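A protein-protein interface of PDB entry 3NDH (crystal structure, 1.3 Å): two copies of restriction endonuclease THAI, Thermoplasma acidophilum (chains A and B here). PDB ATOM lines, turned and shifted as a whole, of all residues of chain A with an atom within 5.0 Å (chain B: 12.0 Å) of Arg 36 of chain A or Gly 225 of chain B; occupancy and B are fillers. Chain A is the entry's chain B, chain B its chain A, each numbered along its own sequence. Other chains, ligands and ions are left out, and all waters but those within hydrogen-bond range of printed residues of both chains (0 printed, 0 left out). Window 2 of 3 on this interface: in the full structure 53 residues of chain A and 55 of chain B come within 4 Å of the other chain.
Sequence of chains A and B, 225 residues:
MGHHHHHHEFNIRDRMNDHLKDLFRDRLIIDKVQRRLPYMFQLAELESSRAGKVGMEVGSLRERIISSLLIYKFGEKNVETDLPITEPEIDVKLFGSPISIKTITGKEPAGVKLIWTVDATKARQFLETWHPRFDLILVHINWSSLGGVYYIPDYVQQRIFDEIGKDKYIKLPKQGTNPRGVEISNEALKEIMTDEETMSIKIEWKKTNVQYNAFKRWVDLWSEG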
ATOM      1  N   ASP A  31     -34.619  -6.337 -29.066  1.00  0.00           N
ATOM      2  CA  ASP A  31     -35.300  -5.597 -28.013  1.00  0.00           C
ATOM      3  C   ASP A  31     -34.610  -5.757 -26.651  1.00  0.00           C
ATOM      4  O   ASP A  31     -34.363  -4.775 -25.945  1.00  0.00           O
ATOM      5  CB  ASP A  31     -36.784  -6.008 -27.949  1.00  0.00           C
ATOM      6  CG  ASP A  31     -37.596  -5.428 -29.092  1.00  0.00           C
ATOM      7  OD1 ASP A  31     -37.127  -4.447 -29.709  1.00  0.00           O
ATOM      8  OD2 ASP A  31     -38.711  -5.933 -29.375  1.00  0.00           O
ATOM      9  N   LYS A  32     -34.256  -6.987 -26.289  1.00  0.00           N
ATOM     10  CA  LYS A  32     -33.522  -7.242 -25.031  1.00  0.00           C
ATOM     11  C   LYS A  32     -32.162  -6.544 -25.039  1.00  0.00           C
ATOM     12  O   LYS A  32     -31.772  -5.945 -24.051  1.00  0.00           O
ATOM     13  CB  LYS A  32     -33.331  -8.739 -24.729  1.00  0.00           C
ATOM     14  CG  LYS A  32     -34.467  -9.380 -23.938  1.00  0.00           C
ATOM     15  CD  LYS A  32     -34.079 -10.768 -23.437  1.00  0.00           C
ATOM     16  CE  LYS A  32     -35.136 -11.327 -22.488  1.00  0.00           C
ATOM     17  NZ  LYS A  32     -34.679 -12.564 -21.777  1.00  0.00           N
ATOM     18  N   VAL A  33     -31.460  -6.584 -26.165  1.00  0.00           N
ATOM     19  CA  VAL A  33     -30.171  -5.878 -26.285  1.00  0.00           C
ATOM     20  C   VAL A  33     -30.343  -4.366 -26.074  1.00  0.00           C
ATOM     21  O   VAL A  33     -29.622  -3.737 -25.278  1.00  0.00           O
ATOM     22  CB  VAL A  33     -29.516  -6.161 -27.639  1.00  0.00           C
ATOM     23  CG1 VAL A  33     -28.243  -5.310 -27.818  1.00  0.00           C
ATOM     24  CG2 VAL A  33     -29.171  -7.662 -27.743  1.00  0.00           C
ATOM     25  N   GLN A  34     -31.343  -3.774 -26.720  1.00  0.00           N
ATOM     26  CA  GLN A  34     -31.588  -2.352 -26.580  1.00  0.00           C
ATOM     27  C   GLN A  34     -31.977  -1.951 -25.165  1.00  0.00           C
ATOM     28  O   GLN A  34     -31.607  -0.871 -24.694  1.00  0.00           O
ATOM     29  CB  GLN A  34     -32.639  -1.907 -27.613  1.00  0.00           C
ATOM     30  CG  GLN A  34     -32.131  -1.952 -29.040  1.00  0.00           C
ATOM     31  CD  GLN A  34     -33.159  -1.604 -30.059  1.00  0.00           C
ATOM     32  OE1 GLN A  34     -34.339  -1.903 -29.881  1.00  0.00           O
ATOM     33  NE2 GLN A  34     -32.725  -0.962 -31.144  1.00  0.00           N
ATOM     34  N   ARG A  35     -32.714  -2.812 -24.474  1.00  0.00           N
ATOM     35  CA  ARG A  35     -33.180  -2.517 -23.114  1.00  0.00           C
ATOM     36  C   ARG A  35     -32.162  -2.803 -22.010  1.00  0.00           C
ATOM     37  O   ARG A  35     -32.213  -2.186 -20.945  1.00  0.00           O
ATOM     38  CB  ARG A  35     -34.455  -3.292 -22.829  1.00  0.00           C
ATOM     39  CG  ARG A  35     -35.615  -2.784 -23.642  1.00  0.00           C
ATOM     40  CD  ARG A  35     -36.873  -3.602 -23.406  1.00  0.00           C
ATOM     41  NE  ARG A  35     -38.011  -3.274 -24.279  1.00  0.00           N
ATOM     42  CZ  ARG A  35     -37.961  -2.983 -25.583  1.00  0.00           C
ATOM     43  NH1 ARG A  35     -36.817  -2.950 -26.267  1.00  0.00           N
ATOM     44  NH2 ARG A  35     -39.089  -2.720 -26.230  1.00  0.00           N
ATOM     45  N   ARG A  36     -31.231  -3.715 -22.269  1.00  0.00           N
ATOM     46  CA  ARG A  36     -30.320  -4.199 -21.223  1.00  0.00           C
ATOM     47  C   ARG A  36     -28.844  -3.941 -21.424  1.00  0.00           C
ATOM     48  O   ARG A  36     -28.102  -3.944 -20.419  1.00  0.00           O
ATOM     49  CB  ARG A  36     -30.535  -5.692 -21.033  1.00  0.00           C
ATOM     50  CG  ARG A  36     -31.965  -6.043 -20.775  1.00  0.00           C
ATOM     51  CD  ARG A  36     -32.133  -7.512 -20.484  1.00  0.00           C
ATOM     52  NE  ARG A  36     -33.528  -7.795 -20.173  1.00  0.00           N
ATOM     53  CZ  ARG A  36     -33.974  -8.971 -19.735  1.00  0.00           C
ATOM     54  NH1 ARG A  36     -33.128  -9.973 -19.539  1.00  0.00           N
ATOM     55  NH2 ARG A  36     -35.268  -9.111 -19.484  1.00  0.00           N
ATOM     56  N   LEU A  37     -28.405  -3.744 -22.670  1.00  0.00           N
ATOM     57  CA  LEU A  37     -26.977  -3.529 -22.892  1.00  0.00           C
ATOM     58  C   LEU A  37     -26.426  -2.320 -22.108  1.00  0.00           C
ATOM     59  O   LEU A  37     -25.356  -2.413 -21.502  1.00  0.00           O
ATOM     60  CB  LEU A  37     -26.619  -3.486 -24.383  1.00  0.00           C
ATOM     61  CG  LEU A  37     -25.134  -3.655 -24.652  1.00  0.00           C
ATOM     62  CD1 LEU A  37     -24.602  -5.017 -24.290  1.00  0.00           C
ATOM     63  CD2 LEU A  37     -24.898  -3.384 -26.114  1.00  0.00           C
ATOM     64  N   PRO A  38     -27.118  -1.176 -22.128  1.00  0.00           N
ATOM     65  CA  PRO A  38     -26.572  -0.047 -21.350  1.00  0.00           C
ATOM     66  C   PRO A  38     -26.378  -0.349 -19.861  1.00  0.00           C
ATOM     67  O   PRO A  38     -25.324  -0.045 -19.308  1.00  0.00           O
ATOM     68  CB  PRO A  38     -27.595   1.086 -21.617  1.00  0.00           C
ATOM     69  CG  PRO A  38     -28.234   0.696 -22.917  1.00  0.00           C
ATOM     70  CD  PRO A  38     -28.345  -0.789 -22.856  1.00  0.00           C
ATOM     71  N   TYR A  39     -27.358  -1.002 -19.230  1.00  0.00           N
ATOM     72  CA  TYR A  39     -27.250  -1.370 -17.829  1.00  0.00           C
ATOM     73  C   TYR A  39     -26.019  -2.225 -17.587  1.00  0.00           C
ATOM     74  O   TYR A  39     -25.264  -1.976 -16.646  1.00  0.00           O
ATOM     75  CB  TYR A  39     -28.515  -2.121 -17.385  1.00  0.00           C
ATOM     76  CG  TYR A  39     -28.439  -2.673 -15.985  1.00  0.00           C
ATOM     77  CD1 TYR A  39     -28.473  -1.841 -14.887  1.00  0.00           C
ATOM     78  CD2 TYR A  39     -28.319  -4.042 -15.771  1.00  0.00           C
ATOM     79  CE1 TYR A  39     -28.392  -2.359 -13.589  1.00  0.00           C
ATOM     80  CE2 TYR A  39     -28.255  -4.572 -14.485  1.00  0.00           C
ATOM     81  CZ  TYR A  39     -28.284  -3.722 -13.404  1.00  0.00           C
ATOM     82  OH  TYR A  39     -28.214  -4.212 -12.103  1.00  0.00           O
ATOM     83  N   MET A  40     -25.871  -3.293 -18.361  1.00  0.00           N
ATOM     84  CA  MET A  40     -24.751  -4.187 -18.172  1.00  0.00           C
ATOM     85  C   MET A  40     -23.419  -3.470 -18.391  1.00  0.00           C
ATOM     86  O   MET A  40     -22.456  -3.683 -17.651  1.00  0.00           O
ATOM     87  CB  MET A  40     -24.845  -5.397 -19.088  1.00  0.00           C
ATOM     88  CG  MET A  40     -26.069  -6.247 -18.827  1.00  0.00           C
ATOM     89  SD  MET A  40     -25.939  -7.898 -19.560  1.00  0.00           S
ATOM     90  CE  MET A  40     -27.676  -8.264 -19.841  1.00  0.00           C
ATOM     91  N   LYS B 216     -21.488 -16.723 -16.186  1.00  0.00           N
ATOM     92  CA  LYS B 216     -22.815 -17.082 -15.684  1.00  0.00           C
ATOM     93  C   LYS B 216     -23.647 -15.858 -15.308  1.00  0.00           C
ATOM     94  O   LYS B 216     -24.819 -15.756 -15.686  1.00  0.00           O
ATOM     95  CB  LYS B 216     -22.703 -18.033 -14.497  1.00  0.00           C
ATOM     96  CG  LYS B 216     -24.057 -18.409 -13.913  1.00  0.00           C
ATOM     97  CD  LYS B 216     -23.904 -19.293 -12.682  1.00  0.00           C
ATOM     98  CE  LYS B 216     -25.110 -19.203 -11.765  1.00  0.00           C
ATOM     99  NZ  LYS B 216     -26.372 -19.506 -12.443  1.00  0.00           N
ATOM    100  N   ARG B 217     -23.039 -14.909 -14.600  1.00  0.00           N
ATOM    101  CA  ARG B 217     -23.760 -13.718 -14.168  1.00  0.00           C
ATOM    102  C   ARG B 217     -24.428 -13.012 -15.340  1.00  0.00           C
ATOM    103  O   ARG B 217     -25.575 -12.565 -15.251  1.00  0.00           O
ATOM    104  CB  ARG B 217     -22.787 -12.778 -13.467  1.00  0.00           C
ATOM    105  CG  ARG B 217     -23.295 -11.410 -13.188  1.00  0.00           C
ATOM    106  CD  ARG B 217     -22.121 -10.576 -12.701  1.00  0.00           C
ATOM    107  NE  ARG B 217     -22.559  -9.248 -12.341  1.00  0.00           N
ATOM    108  CZ  ARG B 217     -21.744  -8.241 -12.044  1.00  0.00           C
ATOM    109  NH1 ARG B 217     -20.429  -8.407 -12.092  1.00  0.00           N
ATOM    110  NH2 ARG B 217     -22.265  -7.067 -11.736  1.00  0.00           N
ATOM    111  N   TRP B 218     -23.689 -12.876 -16.436  1.00  0.00           N
ATOM    112  CA  TRP B 218     -24.143 -12.123 -17.577  1.00  0.00           C
ATOM    113  C   TRP B 218     -25.120 -12.923 -18.419  1.00  0.00           C
ATOM    114  O   TRP B 218     -26.095 -12.347 -18.888  1.00  0.00           O
ATOM    115  CB  TRP B 218     -22.941 -11.636 -18.381  1.00  0.00           C
ATOM    116  CG  TRP B 218     -21.948 -10.886 -17.562  1.00  0.00           C
ATOM    117  CD1 TRP B 218     -20.723 -11.329 -17.204  1.00  0.00           C
ATOM    118  CD2 TRP B 218     -22.118  -9.608 -16.930  1.00  0.00           C
ATOM    119  NE1 TRP B 218     -20.090 -10.393 -16.404  1.00  0.00           N
ATOM    120  CE2 TRP B 218     -20.928  -9.327 -16.231  1.00  0.00           C
ATOM    121  CE3 TRP B 218     -23.145  -8.661 -16.918  1.00  0.00           C
ATOM    122  CZ2 TRP B 218     -20.750  -8.152 -15.505  1.00  0.00           C
ATOM    123  CZ3 TRP B 218     -22.966  -7.495 -16.198  1.00  0.00           C
ATOM    124  CH2 TRP B 218     -21.776  -7.249 -15.510  1.00  0.00           C
ATOM    125  N   VAL B 219     -24.881 -14.220 -18.607  1.00  0.00           N
ATOM    126  CA  VAL B 219     -25.839 -15.060 -19.336  1.00  0.00           C
ATOM    127  C   VAL B 219     -27.185 -15.011 -18.613  1.00  0.00           C
ATOM    128  O   VAL B 219     -28.236 -14.871 -19.241  1.00  0.00           O
ATOM    129  CB  VAL B 219     -25.352 -16.518 -19.503  1.00  0.00           C
ATOM    130  CG1 VAL B 219     -26.440 -17.395 -20.174  1.00  0.00           C
ATOM    131  CG2 VAL B 219     -24.075 -16.550 -20.351  1.00  0.00           C
ATOM    132  N   ASP B 220     -27.131 -15.061 -17.282  1.00  0.00           N
ATOM    133  CA  ASP B 220     -28.351 -14.988 -16.461  1.00  0.00           C
ATOM    134  C   ASP B 220     -29.053 -13.637 -16.617  1.00  0.00           C
ATOM    135  O   ASP B 220     -30.280 -13.582 -16.715  1.00  0.00           O
ATOM    136  CB  ASP B 220     -28.077 -15.320 -14.979  1.00  0.00           C
ATOM    137  CG  ASP B 220     -27.737 -16.777 -14.752  1.00  0.00           C
ATOM    138  OD1 ASP B 220     -27.869 -17.609 -15.674  1.00  0.00           O
ATOM    139  OD2 ASP B 220     -27.341 -17.107 -13.615  1.00  0.00           O
ATOM    140  N   LEU B 221     -28.305 -12.538 -16.658  1.00  0.00           N
ATOM    141  CA  LEU B 221     -28.923 -11.241 -16.917  1.00  0.00           C
ATOM    142  C   LEU B 221     -29.548 -11.129 -18.302  1.00  0.00           C
ATOM    143  O   LEU B 221     -30.551 -10.433 -18.457  1.00  0.00           O
ATOM    144  CB  LEU B 221     -27.927 -10.090 -16.694  1.00  0.00           C
ATOM    145  CG  LEU B 221     -27.571  -9.800 -15.234  1.00  0.00           C
ATOM    146  CD1 LEU B 221     -26.498  -8.732 -15.152  1.00  0.00           C
ATOM    147  CD2 LEU B 221     -28.811  -9.364 -14.438  1.00  0.00           C
ATOM    148  N   TRP B 222     -28.974 -11.793 -19.304  1.00  0.00           N
ATOM    149  CA  TRP B 222     -29.612 -11.875 -20.624  1.00  0.00           C
ATOM    150  C   TRP B 222     -30.893 -12.705 -20.579  1.00  0.00           C
ATOM    151  O   TRP B 222     -31.903 -12.330 -21.178  1.00  0.00           O
ATOM    152  CB  TRP B 222     -28.664 -12.427 -21.707  1.00  0.00           C
ATOM    153  CG  TRP B 222     -27.616 -11.442 -22.105  1.00  0.00           C
ATOM    154  CD1 TRP B 222     -26.272 -11.549 -21.908  1.00  0.00           C
ATOM    155  CD2 TRP B 222     -27.841 -10.172 -22.713  1.00  0.00           C
ATOM    156  NE1 TRP B 222     -25.631 -10.420 -22.384  1.00  0.00           N
ATOM    157  CE2 TRP B 222     -26.580  -9.555 -22.872  1.00  0.00           C
ATOM    158  CE3 TRP B 222     -28.990  -9.492 -23.138  1.00  0.00           C
ATOM    159  CZ2 TRP B 222     -26.443  -8.307 -23.460  1.00  0.00           C
ATOM    160  CZ3 TRP B 222     -28.855  -8.241 -23.690  1.00  0.00           C
ATOM    161  CH2 TRP B 222     -27.586  -7.654 -23.840  1.00  0.00           C
ATOM    162  N   SER B 223     -30.850 -13.816 -19.859  1.00  0.00           N
ATOM    163  CA  SER B 223     -31.912 -14.799 -19.911  1.00  0.00           C
ATOM    164  C   SER B 223     -33.132 -14.426 -19.099  1.00  0.00           C
ATOM    165  O   SER B 223     -34.259 -14.699 -19.490  1.00  0.00           O
ATOM    166  CB  SER B 223     -31.364 -16.150 -19.468  1.00  0.00           C
ATOM    167  OG  SER B 223     -32.379 -17.147 -19.593  1.00  0.00           O
ATOM    168  N   GLU B 224     -32.921 -13.786 -17.961  1.00  0.00           N
ATOM    169  CA  GLU B 224     -34.025 -13.578 -17.032  1.00  0.00           C
ATOM    170  C   GLU B 224     -35.101 -12.658 -17.611  1.00  0.00           C
ATOM    171  O   GLU B 224     -34.809 -11.740 -18.367  1.00  0.00           O
ATOM    172  CB  GLU B 224     -33.512 -13.065 -15.682  1.00  0.00           C
ATOM    173  CG  GLU B 224     -32.837 -11.710 -15.715  1.00  0.00           C
ATOM    174  CD  GLU B 224     -32.481 -11.198 -14.325  1.00  0.00           C
ATOM    175  OE1 GLU B 224     -32.099 -12.015 -13.461  1.00  0.00           O
ATOM    176  OE2 GLU B 224     -32.584  -9.975 -14.094  1.00  0.00           O
ATOM    177  N   GLY B 225     -36.346 -12.928 -17.252  1.00  0.00           N
ATOM    178  CA  GLY B 225     -37.480 -12.130 -17.680  1.00  0.00           C
ATOM    179  C   GLY B 225     -37.684 -12.074 -19.169  1.00  0.00           C
ATOM    180  O   GLY B 225     -37.298 -12.994 -19.928  1.00  0.00           O
ATOM    181  OXT GLY B 225     -38.257 -11.082 -19.633  1.00  0.00           O
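Asp 31 of chain A touches none of the printed residues of chain B.
Printed residues of chain B within 4 Å of Lys 32 of chain A: Trp 222, Ser 223, Glu 224 and Gly 225.
Val 33 of chain A touches one residue of chain B.
Of the printed residues of chain B, Arg 36 of chain A touches Leu 221 (2.8 Å), Trp 222 (3.1 Å), Glu 224 (2.7 Å) and Gly 225 (3.6 Å).
No residue of chain B comes within 4 Å of Pro 38 of chain A.
Of the printed residues of chain B, Met 40 of chain A touches Trp 218, Leu 221 and Trp 222.
Printed residues of chain A within 4 Å of Trp 218 of chain B: Met 40 (3.9 Å).
Val 219 of chain B touches none of the printed residues of chain A.
Of the printed residues of chain A, Leu 221 of chain B touches Arg 36 and Met 40.
Gly 225 of chain B touches just these residues of chain A: Lys 32 (3.2 Å) and Arg 36 (3.6 Å).
The nearest printed residue of chain A that does not touch Leu 221 of chain B is Tyr 39 of chain A (4.6 Å).
Among the printed residues, pairs that only touch across the chains: Lys 32 of chain A with Glu 224 of chain B, Val 33 of chain A with Trp 222 of chain B, Leu 37 of chain A with Trp 222 of chain B, Met 40 of chain A with Trp 218 of chain B and Met 40 of chain A with Leu 221 of chain B.
O of Leu 221 of chain B lies within hydrogen-bond range of NH1 of Arg 36 of chain A (2.8 Å).
The backbone carbonyl oxygen of Trp 222 of chain B is in hydrogen-bond range of the side-chain amino group of Lys 32 of chain A, 2.8 Å away.
The backbone carbonyl oxygen (O) of Trp 222 of chain B is in hydrogen-bond range of the guanidinium group (NH1) of Arg 36 of chain A, 3.1 Å away.
NE1 of Trp 222 of chain B sits close to SD of Met 40 of chain A (3.8 Å).
NZ of Lys 32 of chain A lies within hydrogen-bond range of O of Ser 223 of chain B.
O of Glu 224 of chain B is in hydrogen-bond range of NH1 of Arg 36 of chain A (2.7 Å).
The chain-end carboxylate of Gly 225 of chain B lies within salt-bridge range of the side-chain amino group of Lys 32 of chain A, at 3.2 Å.
The chain-end carboxylate (OXT) of Gly 225 of chain B is in salt-bridge range of the guanidinium group (NH2) of Arg 36 of chain A, at 3.6 Å.
No position is printed for both chains.
Printed residues of chain A that touch a printed residue of chain B: Lys 32, Val 33, Arg 36, Leu 37 and Met 40.
Among the printed residues, 13 pairs touch across the chains.
Among the printed residues, no Asp or Glu carboxylate lies within 4 Å of a Lys or Arg side-chain nitrogen of the other chain.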
